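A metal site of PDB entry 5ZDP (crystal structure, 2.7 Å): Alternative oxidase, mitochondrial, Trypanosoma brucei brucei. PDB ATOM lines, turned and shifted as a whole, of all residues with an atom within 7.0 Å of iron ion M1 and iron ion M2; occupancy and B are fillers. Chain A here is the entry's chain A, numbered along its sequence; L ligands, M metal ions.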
ATOM      1  N   CYS A 119      22.186  22.115 -19.376  1.00  0.00           N
ATOM      2  CA  CYS A 119      21.081  22.676 -18.599  1.00  0.00           C
ATOM      3  C   CYS A 119      20.719  21.840 -17.365  1.00  0.00           C
ATOM      4  O   CYS A 119      20.235  22.364 -16.356  1.00  0.00           O
ATOM      5  CB  CYS A 119      19.852  22.827 -19.513  1.00  0.00           C
ATOM      6  SG  CYS A 119      20.218  23.667 -21.062  1.00  0.00           S
ATOM      7  N   LEU A 122      23.664  23.233 -15.081  1.00  0.00           N
ATOM      8  CA  LEU A 122      23.506  24.641 -14.733  1.00  0.00           C
ATOM      9  C   LEU A 122      22.262  24.935 -13.898  1.00  0.00           C
ATOM     10  O   LEU A 122      22.227  25.924 -13.171  1.00  0.00           O
ATOM     11  CB  LEU A 122      23.541  25.502 -15.998  1.00  0.00           C
ATOM     12  CG  LEU A 122      24.924  25.572 -16.666  1.00  0.00           C
ATOM     13  CD1 LEU A 122      24.932  26.291 -18.007  1.00  0.00           C
ATOM     14  CD2 LEU A 122      25.923  26.231 -15.715  1.00  0.00           C
ATOM     15  N   GLU A 123      21.259  24.070 -13.979  1.00  0.00           N
ATOM     16  CA  GLU A 123      20.045  24.222 -13.163  1.00  0.00           C
ATOM     17  C   GLU A 123      20.196  23.685 -11.750  1.00  0.00           C
ATOM     18  O   GLU A 123      19.398  24.027 -10.866  1.00  0.00           O
ATOM     19  CB  GLU A 123      18.830  23.552 -13.829  1.00  0.00           C
ATOM     20  CG  GLU A 123      18.378  24.237 -15.122  1.00  0.00           C
ATOM     21  CD  GLU A 123      17.843  25.653 -14.938  1.00  0.00           C
ATOM     22  OE1 GLU A 123      17.572  26.335 -15.950  1.00  0.00           O
ATOM     23  OE2 GLU A 123      17.668  26.085 -13.782  1.00  0.00           O
ATOM     24  N   ALA A 126      21.305  26.921 -10.220  1.00  0.00           N
ATOM     25  CA  ALA A 126      20.275  27.949 -10.299  1.00  0.00           C
ATOM     26  C   ALA A 126      19.301  27.859  -9.146  1.00  0.00           C
ATOM     27  O   ALA A 126      18.805  28.858  -8.627  1.00  0.00           O
ATOM     28  CB  ALA A 126      19.520  27.830 -11.618  1.00  0.00           C
ATOM     29  N   GLY A 127      19.027  26.641  -8.718  1.00  0.00           N
ATOM     30  CA  GLY A 127      18.159  26.419  -7.576  1.00  0.00           C
ATOM     31  C   GLY A 127      18.764  26.763  -6.237  1.00  0.00           C
ATOM     32  O   GLY A 127      18.039  26.735  -5.239  1.00  0.00           O
ATOM     33  N   GLU A 158      11.083  31.241  -7.015  1.00  0.00           N
ATOM     34  CA  GLU A 158      12.109  31.271  -8.033  1.00  0.00           C
ATOM     35  C   GLU A 158      12.952  30.005  -7.871  1.00  0.00           C
ATOM     36  O   GLU A 158      13.123  29.239  -8.814  1.00  0.00           O
ATOM     37  CB  GLU A 158      12.953  32.548  -7.897  1.00  0.00           C
ATOM     38  CG  GLU A 158      14.215  32.570  -8.751  1.00  0.00           C
ATOM     39  CD  GLU A 158      14.806  33.964  -8.873  1.00  0.00           C
ATOM     40  OE1 GLU A 158      14.064  34.907  -9.297  1.00  0.00           O
ATOM     41  OE2 GLU A 158      16.029  34.103  -8.548  1.00  0.00           O
ATOM     42  N   ASN A 161      11.004  27.150  -8.924  1.00  0.00           N
ATOM     43  CA  ASN A 161      10.892  27.175 -10.365  1.00  0.00           C
ATOM     44  C   ASN A 161      12.178  26.628 -10.950  1.00  0.00           C
ATOM     45  O   ASN A 161      12.143  25.772 -11.829  1.00  0.00           O
ATOM     46  CB  ASN A 161      10.658  28.594 -10.883  1.00  0.00           C
ATOM     47  CG  ASN A 161      10.766  28.687 -12.406  1.00  0.00           C
ATOM     48  OD1 ASN A 161      11.743  29.207 -12.969  1.00  0.00           O
ATOM     49  ND2 ASN A 161       9.753  28.158 -13.085  1.00  0.00           N
ATOM     50  N   GLU A 162      13.322  27.117 -10.488  1.00  0.00           N
ATOM     51  CA  GLU A 162      14.575  26.705 -11.089  1.00  0.00           C
ATOM     52  C   GLU A 162      14.755  25.190 -10.928  1.00  0.00           C
ATOM     53  O   GLU A 162      15.295  24.526 -11.810  1.00  0.00           O
ATOM     54  CB  GLU A 162      15.797  27.477 -10.551  1.00  0.00           C
ATOM     55  CG  GLU A 162      15.915  28.932 -10.995  1.00  0.00           C
ATOM     56  CD  GLU A 162      16.253  29.134 -12.486  1.00  0.00           C
ATOM     57  OE1 GLU A 162      16.056  28.199 -13.306  1.00  0.00           O
ATOM     58  OE2 GLU A 162      16.692  30.255 -12.854  1.00  0.00           O
ATOM     59  N   ARG A 163      14.274  24.637  -9.815  1.00  0.00           N
ATOM     60  CA  ARG A 163      14.378  23.199  -9.570  1.00  0.00           C
ATOM     61  C   ARG A 163      13.345  22.390 -10.405  1.00  0.00           C
ATOM     62  O   ARG A 163      13.530  21.182 -10.640  1.00  0.00           O
ATOM     63  CB  ARG A 163      14.237  22.940  -8.071  1.00  0.00           C
ATOM     64  CG  ARG A 163      14.654  21.555  -7.587  1.00  0.00           C
ATOM     65  CD  ARG A 163      14.238  21.350  -6.134  1.00  0.00           C
ATOM     66  NE  ARG A 163      12.794  21.539  -5.953  1.00  0.00           N
ATOM     67  CZ  ARG A 163      11.867  20.571  -6.001  1.00  0.00           C
ATOM     68  NH1 ARG A 163      10.580  20.890  -5.828  1.00  0.00           N
ATOM     69  NH2 ARG A 163      12.202  19.306  -6.245  1.00  0.00           N
ATOM     70  N   HIS A 165      12.808  23.212 -13.507  1.00  0.00           N
ATOM     71  CA  HIS A 165      13.615  23.124 -14.700  1.00  0.00           C
ATOM     72  C   HIS A 165      14.489  21.881 -14.655  1.00  0.00           C
ATOM     73  O   HIS A 165      14.651  21.207 -15.664  1.00  0.00           O
ATOM     74  CB  HIS A 165      14.500  24.338 -14.822  1.00  0.00           C
ATOM     75  CG  HIS A 165      13.752  25.605 -15.039  1.00  0.00           C
ATOM     76  ND1 HIS A 165      14.368  26.832 -15.127  1.00  0.00           N
ATOM     77  CD2 HIS A 165      12.436  25.836 -15.208  1.00  0.00           C
ATOM     78  CE1 HIS A 165      13.462  27.760 -15.346  1.00  0.00           C
ATOM     79  NE2 HIS A 165      12.279  27.180 -15.408  1.00  0.00           N
ATOM     80  N   LEU A 166      15.060  21.583 -13.483  1.00  0.00           N
ATOM     81  CA  LEU A 166      15.914  20.400 -13.310  1.00  0.00           C
ATOM     82  C   LEU A 166      15.072  19.129 -13.323  1.00  0.00           C
ATOM     83  O   LEU A 166      15.443  18.145 -13.985  1.00  0.00           O
ATOM     84  CB  LEU A 166      16.647  20.487 -11.977  1.00  0.00           C
ATOM     85  CG  LEU A 166      18.056  19.947 -11.767  1.00  0.00           C
ATOM     86  CD1 LEU A 166      18.104  19.171 -10.468  1.00  0.00           C
ATOM     87  CD2 LEU A 166      18.574  19.096 -12.896  1.00  0.00           C
ATOM     88  N   PHE A 169      14.503  18.496 -16.809  1.00  0.00           N
ATOM     89  CA  PHE A 169      15.653  17.998 -17.563  1.00  0.00           C
ATOM     90  C   PHE A 169      16.061  16.595 -17.121  1.00  0.00           C
ATOM     91  O   PHE A 169      16.296  15.719 -17.954  1.00  0.00           O
ATOM     92  CB  PHE A 169      16.822  18.965 -17.455  1.00  0.00           C
ATOM     93  CG  PHE A 169      16.628  20.270 -18.208  1.00  0.00           C
ATOM     94  CD1 PHE A 169      16.328  20.265 -19.570  1.00  0.00           C
ATOM     95  CD2 PHE A 169      16.829  21.486 -17.578  1.00  0.00           C
ATOM     96  CE1 PHE A 169      16.178  21.463 -20.273  1.00  0.00           C
ATOM     97  CE2 PHE A 169      16.689  22.680 -18.262  1.00  0.00           C
ATOM     98  CZ  PHE A 169      16.375  22.661 -19.620  1.00  0.00           C
ATOM     99  N   VAL A 209      23.047  36.868 -10.065  1.00  0.00           N
ATOM    100  CA  VAL A 209      21.968  36.062 -10.654  1.00  0.00           C
ATOM    101  C   VAL A 209      21.337  36.789 -11.849  1.00  0.00           C
ATOM    102  O   VAL A 209      21.107  36.202 -12.917  1.00  0.00           O
ATOM    103  CB  VAL A 209      20.871  35.697  -9.610  1.00  0.00           C
ATOM    104  CG1 VAL A 209      19.612  35.196 -10.268  1.00  0.00           C
ATOM    105  CG2 VAL A 209      21.385  34.656  -8.633  1.00  0.00           C
ATOM    106  N   LEU A 212      23.587  36.125 -14.596  1.00  0.00           N
ATOM    107  CA  LEU A 212      23.537  34.722 -15.021  1.00  0.00           C
ATOM    108  C   LEU A 212      22.328  34.503 -15.903  1.00  0.00           C
ATOM    109  O   LEU A 212      22.390  33.758 -16.861  1.00  0.00           O
ATOM    110  CB  LEU A 212      23.431  33.778 -13.838  1.00  0.00           C
ATOM    111  CG  LEU A 212      24.694  33.528 -13.033  1.00  0.00           C
ATOM    112  CD1 LEU A 212      24.370  32.662 -11.816  1.00  0.00           C
ATOM    113  CD2 LEU A 212      25.788  32.879 -13.894  1.00  0.00           C
ATOM    114  N   GLU A 213      21.219  35.161 -15.558  1.00  0.00           N
ATOM    115  CA  GLU A 213      19.992  35.037 -16.335  1.00  0.00           C
ATOM    116  C   GLU A 213      20.110  35.683 -17.727  1.00  0.00           C
ATOM    117  O   GLU A 213      19.414  35.270 -18.675  1.00  0.00           O
ATOM    118  CB  GLU A 213      18.797  35.646 -15.571  1.00  0.00           C
ATOM    119  CG  GLU A 213      18.503  35.027 -14.221  1.00  0.00           C
ATOM    120  CD  GLU A 213      18.220  33.527 -14.259  1.00  0.00           C
ATOM    121  OE1 GLU A 213      18.670  32.835 -15.205  1.00  0.00           O
ATOM    122  OE2 GLU A 213      17.579  33.020 -13.310  1.00  0.00           O
ATOM    123  N   ALA A 216      21.594  32.927 -19.537  1.00  0.00           N
ATOM    124  CA  ALA A 216      20.652  31.813 -19.680  1.00  0.00           C
ATOM    125  C   ALA A 216      19.549  32.126 -20.697  1.00  0.00           C
ATOM    126  O   ALA A 216      19.036  31.209 -21.339  1.00  0.00           O
ATOM    127  CB  ALA A 216      20.044  31.435 -18.340  1.00  0.00           C
ATOM    128  N   TYR A 220      19.281  29.538 -23.921  1.00  0.00           N
ATOM    129  CA  TYR A 220      17.937  29.094 -24.345  1.00  0.00           C
ATOM    130  C   TYR A 220      17.435  29.779 -25.617  1.00  0.00           C
ATOM    131  O   TYR A 220      16.586  29.212 -26.287  1.00  0.00           O
ATOM    132  CB  TYR A 220      16.875  29.233 -23.240  1.00  0.00           C
ATOM    133  CG  TYR A 220      17.068  28.279 -22.070  1.00  0.00           C
ATOM    134  CD1 TYR A 220      17.168  26.903 -22.272  1.00  0.00           C
ATOM    135  CD2 TYR A 220      17.120  28.755 -20.763  1.00  0.00           C
ATOM    136  CE1 TYR A 220      17.342  26.029 -21.201  1.00  0.00           C
ATOM    137  CE2 TYR A 220      17.291  27.886 -19.684  1.00  0.00           C
ATOM    138  CZ  TYR A 220      17.396  26.528 -19.909  1.00  0.00           C
ATOM    139  OH  TYR A 220      17.563  25.659 -18.844  1.00  0.00           O
ATOM    140  N   ILE A 262      10.728  27.839 -20.294  1.00  0.00           N
ATOM    141  CA  ILE A 262      11.847  27.866 -19.376  1.00  0.00           C
ATOM    142  C   ILE A 262      12.577  29.213 -19.504  1.00  0.00           C
ATOM    143  O   ILE A 262      12.843  29.904 -18.507  1.00  0.00           O
ATOM    144  CB  ILE A 262      12.795  26.663 -19.572  1.00  0.00           C
ATOM    145  CG1 ILE A 262      12.163  25.428 -18.931  1.00  0.00           C
ATOM    146  CG2 ILE A 262      14.134  26.930 -18.915  1.00  0.00           C
ATOM    147  CD1 ILE A 262      12.820  24.116 -19.281  1.00  0.00           C
ATOM    148  N   ASP A 265      10.844  32.183 -17.713  1.00  0.00           N
ATOM    149  CA  ASP A 265      11.109  32.154 -16.290  1.00  0.00           C
ATOM    150  C   ASP A 265      12.471  32.775 -15.954  1.00  0.00           C
ATOM    151  O   ASP A 265      12.591  33.536 -14.993  1.00  0.00           O
ATOM    152  CB  ASP A 265      11.054  30.711 -15.783  1.00  0.00           C
ATOM    153  CG  ASP A 265       9.634  30.154 -15.767  1.00  0.00           C
ATOM    154  OD1 ASP A 265       8.664  30.942 -15.638  1.00  0.00           O
ATOM    155  OD2 ASP A 265       9.482  28.915 -15.861  1.00  0.00           O
ATOM    156  N   GLU A 266      13.487  32.477 -16.766  1.00  0.00           N
ATOM    157  CA  GLU A 266      14.820  33.062 -16.605  1.00  0.00           C
ATOM    158  C   GLU A 266      14.822  34.577 -16.814  1.00  0.00           C
ATOM    159  O   GLU A 266      15.665  35.267 -16.255  1.00  0.00           O
ATOM    160  CB  GLU A 266      15.853  32.441 -17.582  1.00  0.00           C
ATOM    161  CG  GLU A 266      15.926  30.921 -17.619  1.00  0.00           C
ATOM    162  CD  GLU A 266      16.244  30.271 -16.284  1.00  0.00           C
ATOM    163  OE1 GLU A 266      16.228  29.024 -16.223  1.00  0.00           O
ATOM    164  OE2 GLU A 266      16.498  30.978 -15.277  1.00  0.00           O
ATOM    165  N   HIS A 269      13.401  36.187 -13.788  1.00  0.00           N
ATOM    166  CA  HIS A 269      14.439  36.134 -12.781  1.00  0.00           C
ATOM    167  C   HIS A 269      15.414  37.279 -13.013  1.00  0.00           C
ATOM    168  O   HIS A 269      15.787  37.996 -12.096  1.00  0.00           O
ATOM    169  CB  HIS A 269      15.173  34.799 -12.837  1.00  0.00           C
ATOM    170  CG  HIS A 269      14.296  33.637 -12.520  1.00  0.00           C
ATOM    171  ND1 HIS A 269      14.772  32.344 -12.457  1.00  0.00           N
ATOM    172  CD2 HIS A 269      12.976  33.572 -12.250  1.00  0.00           C
ATOM    173  CE1 HIS A 269      13.765  31.533 -12.173  1.00  0.00           C
ATOM    174  NE2 HIS A 269      12.668  32.265 -12.037  1.00  0.00           N
ATOM    175  N   ARG A 270      15.801  37.409 -14.275  1.00  0.00           N
ATOM    176  CA  ARG A 270      16.642  38.487 -14.748  1.00  0.00           C
ATOM    177  C   ARG A 270      16.066  39.796 -14.178  1.00  0.00           C
ATOM    178  O   ARG A 270      16.708  40.412 -13.337  1.00  0.00           O
ATOM    179  CB  ARG A 270      16.691  38.445 -16.289  1.00  0.00           C
ATOM    180  CG  ARG A 270      17.815  39.228 -16.940  1.00  0.00           C
ATOM    181  CD  ARG A 270      17.755  39.115 -18.458  1.00  0.00           C
ATOM    182  NE  ARG A 270      16.421  39.429 -19.005  1.00  0.00           N
ATOM    183  CZ  ARG A 270      16.024  39.161 -20.247  1.00  0.00           C
ATOM    184  NH1 ARG A 270      16.845  38.589 -21.118  1.00  0.00           N
ATOM    185  NH2 ARG A 270      14.776  39.478 -20.626  1.00  0.00           N
HETATM  186  O1  LIG L   1      18.814  28.593 -14.477  1.00  0.00           O
HETATM  187  O1  LG2 L   2      20.343  31.010 -11.964  1.00  0.00           O
HETATM  188  O2  LG2 L   2      20.827  30.416 -12.914  1.00  0.00           O
HETATM  189  O1  LG3 L   3      24.931  29.441 -20.601  1.00  0.00           O
HETATM  190  C1  LG3 L   3      24.173  29.246 -19.627  1.00  0.00           C
HETATM  191  O2  LG3 L   3      22.992  28.598 -19.856  1.00  0.00           O
HETATM  192  C2  LG3 L   3      22.141  28.344 -18.813  1.00  0.00           C
HETATM  193  C3  LG3 L   3      22.469  28.761 -17.519  1.00  0.00           C
HETATM  194  C4  LG3 L   3      21.589  28.521 -16.483  1.00  0.00           C
HETATM  195  C5  LG3 L   3      20.396  27.861 -16.746  1.00  0.00           C
HETATM  196  C6  LG3 L   3      20.078  27.440 -18.020  1.00  0.00           C
HETATM  197  C7  LG3 L   3      20.941  27.678 -19.073  1.00  0.00           C
HETATM  198  C8  LG3 L   3      23.669  29.434 -17.288  1.00  0.00           C
HETATM  199  O3  LG3 L   3      23.976  29.836 -16.018  1.00  0.00           O
HETATM  200  C9  LG3 L   3      24.529  29.671 -18.355  1.00  0.00           C
HETATM  201  C10 LG3 L   3      25.771  30.443 -18.189  1.00  0.00           C
HETATM  202  C11 LG3 L   3      26.209  30.686 -16.840  1.00  0.00           C
HETATM  203  C12 LG3 L   3      27.498  30.468 -16.576  1.00  0.00           C
HETATM  204  C13 LG3 L   3      28.443  30.274 -17.686  1.00  0.00           C
HETATM  205  C14 LG3 L   3      28.086  30.426 -15.195  1.00  0.00           C
HETATM  206  C15 LG3 L   3      27.945  28.939 -14.788  1.00  0.00           C
HETATM  207  C16 LG3 L   3      29.150  28.363 -14.085  1.00  0.00           C
HETATM  208  C17 LG3 L   3      29.271  28.300 -12.740  1.00  0.00           C
HETATM  209  C18 LG3 L   3      28.229  28.856 -11.811  1.00  0.00           C
HETATM  210  C19 LG3 L   3      30.536  27.715 -12.148  1.00  0.00           C
HETATM  211  C20 LG3 L   3      30.309  26.486 -11.293  1.00  0.00           C
HETATM  212  C21 LG3 L   3      31.452  26.411 -10.284  1.00  0.00           C
HETATM  213  C22 LG3 L   3      32.188  25.300 -10.038  1.00  0.00           C
HETATM  214  C23 LG3 L   3      33.290  25.342  -9.035  1.00  0.00           C
HETATM  215  C24 LG3 L   3      31.941  24.015 -10.763  1.00  0.00           C
HETATM  216 FE    FE M   1      18.098  30.861 -13.839  1.00  0.00          FE
HETATM  217 FE    FE M   2      16.890  27.767 -15.098  1.00  0.00          FE
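Iron ion M1 is bound by the side-chain carboxylate (OE2) of Glu 162, the side-chain carboxylate (OE2) of Glu 266, the side-chain carboxylate (OE2) of Glu 213, an oxygen (O1) of LIG L1 and the side-chain carboxylate (OE1) of Glu 213.
OE1 of Glu 123 binds iron ion M2 (1.8 Å). The side-chain carboxylate (OE1) of Glu 266 is bound to iron ion M2, at 1.8 Å. Iron ion M2 is bound by OE1 of Glu 162 (2.0 Å). O1 of LIG L1 binds iron ion M2 (2.2 Å). OE2 of Glu 123 binds iron ion M2 (2.3 Å). Slightly farther from iron ion M2 lies a ring nitrogen (ND1) of His 165 (2.7 Å).
Within 4 Å of iron ion M2: Glu 123, Glu 162, His 165 and Glu 266. The nearest printed residue that does not touch iron ion M2 is Tyr 220 (4.4 Å).
His 269 touches iron ion M1. Of the 22 residues printed, 4 come within 4 Å of iron ion M1.
ND1 of His 165 lies close to OE1 of Glu 123, at 3.3 Å. OE1 of Glu 123 sits close to OH of Tyr 220 (3.0 Å). The side-chain carboxylate of Glu 162 sits close to a ring nitrogen (ND1) of His 165, at 2.8 Å. OE2 of Glu 162 lies close to ND1 of His 269, at 2.9 Å. OE2 of Glu 213 sits close to ND1 of His 269, 3.0 Å away. NE2 of His 165 is in hydrogen-bond range of OD1 of Asn 161, 3.2 Å away. OD2 of Asp 265 is in hydrogen-bond range of NE2 of His 165 (3.3 Å). NE2 of His 269 lies close to OD1 of Asn 161.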
